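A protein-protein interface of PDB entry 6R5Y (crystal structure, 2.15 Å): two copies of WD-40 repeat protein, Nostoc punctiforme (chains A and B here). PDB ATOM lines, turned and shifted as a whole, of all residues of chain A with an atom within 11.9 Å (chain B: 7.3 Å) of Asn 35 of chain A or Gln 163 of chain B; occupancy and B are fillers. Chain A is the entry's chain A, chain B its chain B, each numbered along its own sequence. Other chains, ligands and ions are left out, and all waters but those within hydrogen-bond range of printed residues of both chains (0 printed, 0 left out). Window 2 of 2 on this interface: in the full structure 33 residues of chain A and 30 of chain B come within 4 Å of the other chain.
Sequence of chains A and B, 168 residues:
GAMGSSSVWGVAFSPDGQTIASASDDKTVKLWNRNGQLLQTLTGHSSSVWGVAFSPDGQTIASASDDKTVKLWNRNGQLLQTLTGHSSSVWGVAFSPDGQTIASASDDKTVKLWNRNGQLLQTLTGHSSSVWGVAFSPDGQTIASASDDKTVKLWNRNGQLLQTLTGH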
ATOM      1  N   GLY A  10      22.507   7.565   7.623  1.00  0.00           N
ATOM      2  CA  GLY A  10      21.530   8.524   7.128  1.00  0.00           C
ATOM      3  C   GLY A  10      21.788   9.141   5.773  1.00  0.00           C
ATOM      4  O   GLY A  10      21.132  10.094   5.404  1.00  0.00           O
ATOM      5  N   VAL A  11      22.727   8.590   5.027  1.00  0.00           N
ATOM      6  CA  VAL A  11      23.094   9.144   3.753  1.00  0.00           C
ATOM      7  C   VAL A  11      23.276   8.006   2.793  1.00  0.00           C
ATOM      8  O   VAL A  11      23.796   6.962   3.175  1.00  0.00           O
ATOM      9  CB  VAL A  11      24.410   9.935   3.845  1.00  0.00           C
ATOM     10  CG1 VAL A  11      24.991  10.183   2.446  1.00  0.00           C
ATOM     11  CG2 VAL A  11      24.171  11.237   4.536  1.00  0.00           C
ATOM     12  N   PHE A  13      24.669   7.926  -0.832  1.00  0.00           N
ATOM     13  CA  PHE A  13      25.301   8.362  -2.053  1.00  0.00           C
ATOM     14  C   PHE A  13      25.413   7.140  -2.979  1.00  0.00           C
ATOM     15  O   PHE A  13      25.652   6.034  -2.524  1.00  0.00           O
ATOM     16  CB  PHE A  13      26.754   8.804  -1.829  1.00  0.00           C
ATOM     17  CG  PHE A  13      27.007  10.181  -1.258  1.00  0.00           C
ATOM     18  CD1 PHE A  13      26.814  11.318  -2.021  1.00  0.00           C
ATOM     19  CD2 PHE A  13      27.663  10.327  -0.028  1.00  0.00           C
ATOM     20  CE1 PHE A  13      27.146  12.589  -1.541  1.00  0.00           C
ATOM     21  CE2 PHE A  13      27.998  11.592   0.461  1.00  0.00           C
ATOM     22  CZ  PHE A  13      27.727  12.721  -0.298  1.00  0.00           C
ATOM     23  N   SER A  14      25.234   7.353  -4.269  1.00  0.00           N
ATOM     24  CA  SER A  14      25.620   6.372  -5.271  1.00  0.00           C
ATOM     25  C   SER A  14      27.152   6.243  -5.277  1.00  0.00           C
ATOM     26  O   SER A  14      27.843   7.116  -4.756  1.00  0.00           O
ATOM     27  CB  SER A  14      25.148   6.803  -6.644  1.00  0.00           C
ATOM     28  OG  SER A  14      25.794   8.014  -7.018  1.00  0.00           O
ATOM     29  N   ASP A  16      29.450   6.644  -7.445  1.00  0.00           N
ATOM     30  CA  ASP A  16      30.142   7.759  -8.088  1.00  0.00           C
ATOM     31  C   ASP A  16      29.817   9.130  -7.456  1.00  0.00           C
ATOM     32  O   ASP A  16      30.385  10.134  -7.846  1.00  0.00           O
ATOM     33  CB  ASP A  16      29.810   7.778  -9.573  1.00  0.00           C
ATOM     34  CG  ASP A  16      28.336   7.879  -9.838  1.00  0.00           C
ATOM     35  OD1 ASP A  16      27.529   8.046  -8.897  1.00  0.00           O
ATOM     36  OD2 ASP A  16      27.976   7.791 -11.012  1.00  0.00           O
ATOM     37  N   GLY A  17      28.922   9.165  -6.477  1.00  0.00           N
ATOM     38  CA  GLY A  17      28.590  10.414  -5.776  1.00  0.00           C
ATOM     39  C   GLY A  17      27.748  11.393  -6.575  1.00  0.00           C
ATOM     40  O   GLY A  17      27.527  12.521  -6.154  1.00  0.00           O
ATOM     41  N   GLN A  18      27.251  10.944  -7.723  1.00  0.00           N
ATOM     42  CA  GLN A  18      26.449  11.785  -8.610  1.00  0.00           C
ATOM     43  C   GLN A  18      24.960  11.731  -8.298  1.00  0.00           C
ATOM     44  O   GLN A  18      24.194  12.552  -8.755  1.00  0.00           O
ATOM     45  CB  GLN A  18      26.715  11.383 -10.064  1.00  0.00           C
ATOM     46  CG  GLN A  18      28.162  11.607 -10.481  1.00  0.00           C
ATOM     47  CD  GLN A  18      28.769  12.877  -9.868  1.00  0.00           C
ATOM     48  OE1 GLN A  18      28.342  14.017 -10.135  1.00  0.00           O
ATOM     49  NE2 GLN A  18      29.764  12.678  -9.012  1.00  0.00           N
ATOM     50  N   THR A  19      24.529  10.730  -7.549  1.00  0.00           N
ATOM     51  CA  THR A  19      23.125  10.597  -7.190  1.00  0.00           C
ATOM     52  C   THR A  19      23.049  10.434  -5.702  1.00  0.00           C
ATOM     53  O   THR A  19      23.870   9.738  -5.111  1.00  0.00           O
ATOM     54  CB  THR A  19      22.464   9.383  -7.906  1.00  0.00           C
ATOM     55  OG1 THR A  19      22.655   9.503  -9.311  1.00  0.00           O
ATOM     56  CG2 THR A  19      20.950   9.305  -7.644  1.00  0.00           C
ATOM     57  N   ILE A  20      21.986  10.974  -5.119  1.00  0.00           N
ATOM     58  CA  ILE A  20      21.737  10.771  -3.713  1.00  0.00           C
ATOM     59  C   ILE A  20      20.226  10.381  -3.516  1.00  0.00           C
ATOM     60  O   ILE A  20      19.309  10.982  -4.126  1.00  0.00           O
ATOM     61  CB  ILE A  20      22.300  11.932  -2.880  1.00  0.00           C
ATOM     62  CG1 ILE A  20      21.995  11.762  -1.383  1.00  0.00           C
ATOM     63  CG2 ILE A  20      21.735  13.186  -3.450  1.00  0.00           C
ATOM     64  CD1 ILE A  20      23.108  12.232  -0.477  1.00  0.00           C
ATOM     65  N   ALA A  21      19.974   9.340  -2.718  1.00  0.00           N
ATOM     66  CA  ALA A  21      18.618   8.858  -2.414  1.00  0.00           C
ATOM     67  C   ALA A  21      18.188   9.280  -1.028  1.00  0.00           C
ATOM     68  O   ALA A  21      18.979   9.266  -0.078  1.00  0.00           O
ATOM     69  CB  ALA A  21      18.574   7.350  -2.485  1.00  0.00           C
ATOM     70  N   SER A  22      16.942   9.719  -0.907  1.00  0.00           N
ATOM     71  CA  SER A  22      16.412  10.171   0.374  1.00  0.00           C
ATOM     72  C   SER A  22      14.983   9.652   0.571  1.00  0.00           C
ATOM     73  O   SER A  22      14.164   9.694  -0.319  1.00  0.00           O
ATOM     74  CB  SER A  22      16.430  11.725   0.473  1.00  0.00           C
ATOM     75  OG  SER A  22      15.406  12.307  -0.357  1.00  0.00           O
ATOM     76  N   LEU A  31      15.263  10.394  -5.778  1.00  0.00           N
ATOM     77  CA  LEU A  31      16.635  10.451  -6.237  1.00  0.00           C
ATOM     78  C   LEU A  31      16.971  11.840  -6.726  1.00  0.00           C
ATOM     79  O   LEU A  31      16.236  12.415  -7.554  1.00  0.00           O
ATOM     80  CB  LEU A  31      16.833   9.490  -7.375  1.00  0.00           C
ATOM     81  CG  LEU A  31      16.397   8.076  -7.031  1.00  0.00           C
ATOM     82  CD1 LEU A  31      16.698   7.192  -8.208  1.00  0.00           C
ATOM     83  CD2 LEU A  31      17.092   7.559  -5.796  1.00  0.00           C
ATOM     84  N   TRP A  32      18.067  12.381  -6.204  1.00  0.00           N
ATOM     85  CA  TRP A  32      18.499  13.728  -6.558  1.00  0.00           C
ATOM     86  C   TRP A  32      19.876  13.694  -7.189  1.00  0.00           C
ATOM     87  O   TRP A  32      20.648  12.818  -6.879  1.00  0.00           O
ATOM     88  CB  TRP A  32      18.578  14.590  -5.314  1.00  0.00           C
ATOM     89  CG  TRP A  32      17.361  14.530  -4.461  1.00  0.00           C
ATOM     90  CD1 TRP A  32      17.077  13.612  -3.496  1.00  0.00           C
ATOM     91  CD2 TRP A  32      16.260  15.452  -4.486  1.00  0.00           C
ATOM     92  NE1 TRP A  32      15.847  13.882  -2.930  1.00  0.00           N
ATOM     93  CE2 TRP A  32      15.334  15.019  -3.512  1.00  0.00           C
ATOM     94  CE3 TRP A  32      15.968  16.610  -5.242  1.00  0.00           C
ATOM     95  CZ2 TRP A  32      14.129  15.696  -3.281  1.00  0.00           C
ATOM     96  CZ3 TRP A  32      14.766  17.273  -5.017  1.00  0.00           C
ATOM     97  CH2 TRP A  32      13.865  16.818  -4.040  1.00  0.00           C
ATOM     98  N   ASN A  33      20.168  14.626  -8.091  1.00  0.00           N
ATOM     99  CA  ASN A  33      21.542  14.837  -8.509  1.00  0.00           C
ATOM    100  C   ASN A  33      22.195  15.730  -7.476  1.00  0.00           C
ATOM    101  O   ASN A  33      21.537  16.243  -6.566  1.00  0.00           O
ATOM    102  CB  ASN A  33      21.699  15.355  -9.958  1.00  0.00           C
ATOM    103  CG  ASN A  33      21.383  16.830 -10.130  1.00  0.00           C
ATOM    104  OD1 ASN A  33      21.203  17.598  -9.180  1.00  0.00           O
ATOM    105  ND2 ASN A  33      21.301  17.232 -11.389  1.00  0.00           N
ATOM    106  N   ARG A  34      23.495  15.896  -7.617  1.00  0.00           N
ATOM    107  CA  ARG A  34      24.284  16.624  -6.658  1.00  0.00           C
ATOM    108  C   ARG A  34      23.942  18.122  -6.599  1.00  0.00           C
ATOM    109  O   ARG A  34      24.223  18.778  -5.599  1.00  0.00           O
ATOM    110  CB  ARG A  34      25.765  16.362  -6.974  1.00  0.00           C
ATOM    111  CG  ARG A  34      26.737  17.157  -6.144  1.00  0.00           C
ATOM    112  CD  ARG A  34      28.122  16.550  -6.228  1.00  0.00           C
ATOM    113  NE  ARG A  34      29.031  17.252  -5.322  1.00  0.00           N
ATOM    114  CZ  ARG A  34      29.548  18.462  -5.526  1.00  0.00           C
ATOM    115  NH1 ARG A  34      30.385  18.983  -4.626  1.00  0.00           N
ATOM    116  NH2 ARG A  34      29.255  19.156  -6.620  1.00  0.00           N
ATOM    117  N   ASN A  35      23.315  18.635  -7.655  1.00  0.00           N
ATOM    118  CA  ASN A  35      22.845  20.019  -7.735  1.00  0.00           C
ATOM    119  C   ASN A  35      21.464  20.265  -7.149  1.00  0.00           C
ATOM    120  O   ASN A  35      20.927  21.357  -7.264  1.00  0.00           O
ATOM    121  CB  ASN A  35      22.813  20.470  -9.193  1.00  0.00           C
ATOM    122  CG  ASN A  35      24.191  20.506  -9.825  1.00  0.00           C
ATOM    123  OD1 ASN A  35      25.216  20.608  -9.137  1.00  0.00           O
ATOM    124  ND2 ASN A  35      24.229  20.465 -11.151  1.00  0.00           N
ATOM    125  N   GLY A  36      20.893  19.268  -6.491  1.00  0.00           N
ATOM    126  CA  GLY A  36      19.571  19.408  -5.898  1.00  0.00           C
ATOM    127  C   GLY A  36      18.400  19.238  -6.844  1.00  0.00           C
ATOM    128  O   GLY A  36      17.261  19.472  -6.441  1.00  0.00           O
ATOM    129  N   GLN A  37      18.650  18.836  -8.093  1.00  0.00           N
ATOM    130  CA  GLN A  37      17.557  18.539  -9.021  1.00  0.00           C
ATOM    131  C   GLN A  37      16.983  17.121  -8.854  1.00  0.00           C
ATOM    132  O   GLN A  37      17.715  16.157  -8.720  1.00  0.00           O
ATOM    133  CB  GLN A  37      17.964  18.796 -10.476  1.00  0.00           C
ATOM    134  CG  GLN A  37      18.060  20.334 -10.845  1.00  0.00           C
ATOM    135  CD  GLN A  37      16.679  20.912 -11.135  1.00  0.00           C
ATOM    136  OE1 GLN A  37      15.748  20.183 -11.487  1.00  0.00           O
ATOM    137  NE2 GLN A  37      16.546  22.235 -11.023  1.00  0.00           N
ATOM    138  N   LEU A  38      15.663  17.031  -8.811  1.00  0.00           N
ATOM    139  CA  LEU A  38      14.965  15.756  -8.666  1.00  0.00           C
ATOM    140  C   LEU A  38      15.075  14.963  -9.957  1.00  0.00           C
ATOM    141  O   LEU A  38      14.706  15.454 -11.004  1.00  0.00           O
ATOM    142  CB  LEU A  38      13.488  16.013  -8.336  1.00  0.00           C
ATOM    143  CG  LEU A  38      12.586  14.801  -8.107  1.00  0.00           C
ATOM    144  CD1 LEU A  38      13.047  13.951  -6.931  1.00  0.00           C
ATOM    145  CD2 LEU A  38      11.170  15.274  -7.870  1.00  0.00           C
ATOM    146  N   LEU A  39      15.561  13.739  -9.861  1.00  0.00           N
ATOM    147  CA  LEU A  39      15.702  12.842 -11.012  1.00  0.00           C
ATOM    148  C   LEU A  39      14.587  11.783 -11.136  1.00  0.00           C
ATOM    149  O   LEU A  39      14.062  11.580 -12.216  1.00  0.00           O
ATOM    150  CB  LEU A  39      17.029  12.090 -10.932  1.00  0.00           C
ATOM    151  CG  LEU A  39      18.279  12.946 -10.797  1.00  0.00           C
ATOM    152  CD1 LEU A  39      19.472  12.054 -10.547  1.00  0.00           C
ATOM    153  CD2 LEU A  39      18.492  13.785 -12.041  1.00  0.00           C
ATOM    154  N   ARG A  75      17.745   2.277 -10.894  1.00  0.00           N
ATOM    155  CA  ARG A  75      18.105   3.664 -10.874  1.00  0.00           C
ATOM    156  C   ARG A  75      17.197   4.531 -11.739  1.00  0.00           C
ATOM    157  O   ARG A  75      17.149   5.725 -11.534  1.00  0.00           O
ATOM    158  CB  ARG A  75      19.584   3.812 -11.256  1.00  0.00           C
ATOM    159  CG  ARG A  75      20.178   5.115 -10.786  1.00  0.00           C
ATOM    160  CD  ARG A  75      21.629   4.976 -10.374  1.00  0.00           C
ATOM    161  NE  ARG A  75      22.389   6.218 -10.428  1.00  0.00           N
ATOM    162  CZ  ARG A  75      23.679   6.278 -10.087  1.00  0.00           C
ATOM    163  NH1 ARG A  75      24.317   5.178  -9.662  1.00  0.00           N
ATOM    164  NH2 ARG A  75      24.336   7.433 -10.150  1.00  0.00           N
ATOM    165  N   ILE B 143      30.721  16.367   1.204  1.00  0.00           N
ATOM    166  CA  ILE B 143      30.384  15.807   2.501  1.00  0.00           C
ATOM    167  C   ILE B 143      28.865  15.821   2.657  1.00  0.00           C
ATOM    168  O   ILE B 143      28.223  16.800   2.308  1.00  0.00           O
ATOM    169  CB  ILE B 143      31.028  16.649   3.605  1.00  0.00           C
ATOM    170  CG1 ILE B 143      32.540  16.544   3.484  1.00  0.00           C
ATOM    171  CG2 ILE B 143      30.602  16.163   4.981  1.00  0.00           C
ATOM    172  CD1 ILE B 143      33.247  17.820   3.801  1.00  0.00           C
ATOM    173  N   VAL B 152      19.041  16.133   5.122  1.00  0.00           N
ATOM    174  CA  VAL B 152      20.398  15.789   4.770  1.00  0.00           C
ATOM    175  C   VAL B 152      20.964  16.963   3.978  1.00  0.00           C
ATOM    176  O   VAL B 152      20.279  17.526   3.106  1.00  0.00           O
ATOM    177  CB  VAL B 152      20.432  14.552   3.884  1.00  0.00           C
ATOM    178  CG1 VAL B 152      21.853  14.234   3.473  1.00  0.00           C
ATOM    179  CG2 VAL B 152      19.792  13.383   4.614  1.00  0.00           C
ATOM    180  N   LYS B 153      22.190  17.364   4.308  1.00  0.00           N
ATOM    181  CA  LYS B 153      22.822  18.510   3.669  1.00  0.00           C
ATOM    182  C   LYS B 153      24.092  18.076   3.017  1.00  0.00           C
ATOM    183  O   LYS B 153      24.794  17.209   3.544  1.00  0.00           O
ATOM    184  CB  LYS B 153      23.094  19.628   4.676  1.00  0.00           C
ATOM    185  CG  LYS B 153      21.818  20.367   5.073  1.00  0.00           C
ATOM    186  CD  LYS B 153      22.070  21.449   6.120  1.00  0.00           C
ATOM    187  CE  LYS B 153      20.766  22.106   6.564  1.00  0.00           C
ATOM    188  NZ  LYS B 153      20.243  23.018   5.523  1.00  0.00           N
ATOM    189  N   LEU B 154      24.351  18.632   1.841  1.00  0.00           N
ATOM    190  CA  LEU B 154      25.569  18.363   1.091  1.00  0.00           C
ATOM    191  C   LEU B 154      26.449  19.583   1.111  1.00  0.00           C
ATOM    192  O   LEU B 154      25.966  20.687   0.854  1.00  0.00           O
ATOM    193  CB  LEU B 154      25.263  18.012  -0.352  1.00  0.00           C
ATOM    194  CG  LEU B 154      24.336  16.813  -0.550  1.00  0.00           C
ATOM    195  CD1 LEU B 154      24.255  16.509  -2.041  1.00  0.00           C
ATOM    196  CD2 LEU B 154      24.820  15.577   0.200  1.00  0.00           C
ATOM    197  N   TRP B 155      27.720  19.378   1.412  1.00  0.00           N
ATOM    198  CA  TRP B 155      28.664  20.462   1.557  1.00  0.00           C
ATOM    199  C   TRP B 155      29.939  20.190   0.764  1.00  0.00           C
ATOM    200  O   TRP B 155      30.258  19.052   0.498  1.00  0.00           O
ATOM    201  CB  TRP B 155      29.134  20.592   3.000  1.00  0.00           C
ATOM    202  CG  TRP B 155      28.131  20.425   4.042  1.00  0.00           C
ATOM    203  CD1 TRP B 155      27.548  19.267   4.451  1.00  0.00           C
ATOM    204  CD2 TRP B 155      27.555  21.471   4.845  1.00  0.00           C
ATOM    205  NE1 TRP B 155      26.647  19.519   5.436  1.00  0.00           N
ATOM    206  CE2 TRP B 155      26.647  20.860   5.713  1.00  0.00           C
ATOM    207  CE3 TRP B 155      27.734  22.855   4.914  1.00  0.00           C
ATOM    208  CZ2 TRP B 155      25.895  21.586   6.620  1.00  0.00           C
ATOM    209  CZ3 TRP B 155      26.991  23.578   5.844  1.00  0.00           C
ATOM    210  CH2 TRP B 155      26.076  22.944   6.660  1.00  0.00           C
ATOM    211  N   ASN B 156      30.616  21.251   0.360  1.00  0.00           N
ATOM    212  CA  ASN B 156      31.960  21.118  -0.174  1.00  0.00           C
ATOM    213  C   ASN B 156      32.999  21.213   0.963  1.00  0.00           C
ATOM    214  O   ASN B 156      32.666  21.487   2.107  1.00  0.00           O
ATOM    215  CB  ASN B 156      32.210  22.134  -1.300  1.00  0.00           C
ATOM    216  CG  ASN B 156      32.401  23.556  -0.802  1.00  0.00           C
ATOM    217  OD1 ASN B 156      32.579  23.817   0.375  1.00  0.00           O
ATOM    218  ND2 ASN B 156      32.418  24.484  -1.735  1.00  0.00           N
ATOM    219  N   GLN B 160      31.104  25.287   2.395  1.00  0.00           N
ATOM    220  CA  GLN B 160      29.932  25.894   1.803  1.00  0.00           C
ATOM    221  C   GLN B 160      28.825  24.852   1.628  1.00  0.00           C
ATOM    222  O   GLN B 160      29.062  23.727   1.140  1.00  0.00           O
ATOM    223  CB  GLN B 160      30.299  26.574   0.480  1.00  0.00           C
ATOM    224  CG  GLN B 160      31.005  27.914   0.693  1.00  0.00           C
ATOM    225  CD  GLN B 160      31.779  28.366  -0.524  1.00  0.00           C
ATOM    226  OE1 GLN B 160      32.202  27.554  -1.354  1.00  0.00           O
ATOM    227  NE2 GLN B 160      31.976  29.674  -0.639  1.00  0.00           N
ATOM    228  N   LEU B 161      27.610  25.258   1.995  1.00  0.00           N
ATOM    229  CA  LEU B 161      26.432  24.459   1.773  1.00  0.00           C
ATOM    230  C   LEU B 161      26.107  24.440   0.296  1.00  0.00           C
ATOM    231  O   LEU B 161      25.973  25.486  -0.336  1.00  0.00           O
ATOM    232  CB  LEU B 161      25.241  25.019   2.551  1.00  0.00           C
ATOM    233  CG  LEU B 161      23.927  24.223   2.434  1.00  0.00           C
ATOM    234  CD1 LEU B 161      24.092  22.834   3.022  1.00  0.00           C
ATOM    235  CD2 LEU B 161      22.800  24.967   3.115  1.00  0.00           C
ATOM    236  N   LEU B 162      26.000  23.247  -0.265  1.00  0.00           N
ATOM    237  CA  LEU B 162      25.675  23.108  -1.672  1.00  0.00           C
ATOM    238  C   LEU B 162      24.185  22.925  -1.813  1.00  0.00           C
ATOM    239  O   LEU B 162      23.569  23.540  -2.666  1.00  0.00           O
ATOM    240  CB  LEU B 162      26.428  21.919  -2.286  1.00  0.00           C
ATOM    241  CG  LEU B 162      27.961  22.001  -2.201  1.00  0.00           C
ATOM    242  CD1 LEU B 162      28.610  20.704  -2.693  1.00  0.00           C
ATOM    243  CD2 LEU B 162      28.485  23.191  -2.985  1.00  0.00           C
ATOM    244  N   GLN B 163      23.629  21.992  -1.050  1.00  0.00           N
ATOM    245  CA  GLN B 163      22.268  21.586  -1.199  1.00  0.00           C
ATOM    246  C   GLN B 163      21.718  20.944   0.015  1.00  0.00           C
ATOM    247  O   GLN B 163      22.445  20.380   0.789  1.00  0.00           O
ATOM    248  CB  GLN B 163      22.225  20.485  -2.240  1.00  0.00           C
ATOM    249  CG  GLN B 163      22.273  20.948  -3.682  1.00  0.00           C
ATOM    250  CD  GLN B 163      21.213  21.995  -3.969  1.00  0.00           C
ATOM    251  OE1 GLN B 163      20.114  21.989  -3.361  1.00  0.00           O
ATOM    252  NE2 GLN B 163      21.536  22.931  -4.840  1.00  0.00           N
ATOM    253  N   THR B 164      20.396  20.999   0.144  1.00  0.00           N
ATOM    254  CA  THR B 164      19.672  20.360   1.225  1.00  0.00           C
ATOM    255  C   THR B 164      18.607  19.440   0.635  1.00  0.00           C
ATOM    256  O   THR B 164      17.843  19.838  -0.239  1.00  0.00           O
ATOM    257  CB  THR B 164      18.947  21.408   2.102  1.00  0.00           C
ATOM    258  OG1 THR B 164      19.885  22.329   2.634  1.00  0.00           O
ATOM    259  CG2 THR B 164      18.199  20.743   3.257  1.00  0.00           C
ATOM    260  N   LEU B 165      18.563  18.212   1.124  1.00  0.00           N
ATOM    261  CA  LEU B 165      17.476  17.319   0.833  1.00  0.00           C
ATOM    262  C   LEU B 165      16.596  17.415   2.054  1.00  0.00           C
ATOM    263  O   LEU B 165      17.034  17.151   3.203  1.00  0.00           O
ATOM    264  CB  LEU B 165      17.957  15.903   0.606  1.00  0.00           C
ATOM    265  CG  LEU B 165      19.146  15.704  -0.338  1.00  0.00           C
ATOM    266  CD1 LEU B 165      19.439  14.209  -0.389  1.00  0.00           C
ATOM    267  CD2 LEU B 165      18.794  16.203  -1.716  1.00  0.00           C
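NE2 of Gln 163 of chain B sits at hydrogen-bond distance from O of Asn 35 of chain A (3.0 Å).
The backbone carbonyl oxygen (O) of Ile 20 of chain A lies within hydrogen-bond range of the backbone NH (N) of Trp 32 of chain A, 2.8 Å away.
The side-chain hydroxyl (OG) of Ser 22 of chain A sits at hydrogen-bond distance from the indole nitrogen (NE1) of Trp 32 of chain A, at 3.0 Å.
N of Asn 35 of chain A lies within hydrogen-bond range of OD1 of Asn 33 of chain A (2.8 Å).
The side-chain amide oxygen (OD1) of Asn 33 of chain A lies within hydrogen-bond range of the backbone NH (N) of Gly 36 of chain A, at 3.2 Å.
O of Leu 154 of chain B is in hydrogen-bond range of N of Leu 162 of chain B, 2.8 Å away.
The backbone NH of Leu 154 of chain B lies within hydrogen-bond range of the backbone carbonyl oxygen of Gln 163 of chain B.
Gly 10 of chain A touches Val 152 of chain B (O to CG2, 3.6 Å).
Val 152 of chain B touches Val 11 of chain A.
Ile 20 of chain A touches Leu 154 of chain B (CD1 to CD2, 3.8 Å).
Leu 165 of chain B touches Ile 20 of chain A (CD1 to CG1, 3.7 Å).
Leu 165 of chain B touches Ser 22 of chain A.
Trp 32 of chain A touches Leu 165 of chain B (CG to CD2, 3.5 Å).
CD1 of Leu 162 of chain B touches NH1 of Arg 34 of chain A, at 3.1 Å.
Gln 163 of chain B touches Arg 34 of chain A (CG to O, 3.5 Å).
N of Gly 36 of chain A touches CG of Gln 163 of chain B (3.6 Å).
Printed residues of chain B within 4 Å of Ile 20 of chain A: Leu 154 and Leu 165.
Of the printed residues of chain B, Ser 22 of chain A touches Leu 165 (3.996 Å).
Asn 33 of chain A touches none of the printed residues of chain B.
Of chain B, only Gln 163 comes within 4 Å of Asn 35 of chain A.
Of the printed residues of chain A, Val 152 of chain B touches Gly 10 and Val 11.
No residue of chain A comes within 4 Å of Lys 153 of chain B.
Leu 154 of chain B touches just one residue of chain A: Ile 20.
No residue of chain A comes within 4 Å of Leu 161 of chain B.
Leu 162 of chain B touches just one residue of chain A: Arg 34 (3.1 Å).
Of chain A, only Arg 34, Asn 35 and Gly 36 come within 4 Å of Gln 163 of chain B.
No residue of chain A comes within 4 Å of Thr 164 of chain B.
The nearest residue of chain B that does not touch Asn 35 of chain A is Leu 162 of chain B (5.7 Å).
The nearest residue of chain A that does not touch Gln 163 of chain B is Asn 33 of chain A (5.6 Å).
Of the 12 printed residues of chain B, 5 touch a printed residue of chain A.
Among the printed residues, 10 pairs touch across the chains.
Among the printed residues, no Asp or Glu carboxylate lies within 4 Å of a Lys or Arg side-chain nitrogen of the other chain.
No position is printed for both chains.
Of the 10 pairs that touch across the chains among the printed residues, none has its exchanged pair printed and touching as well.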
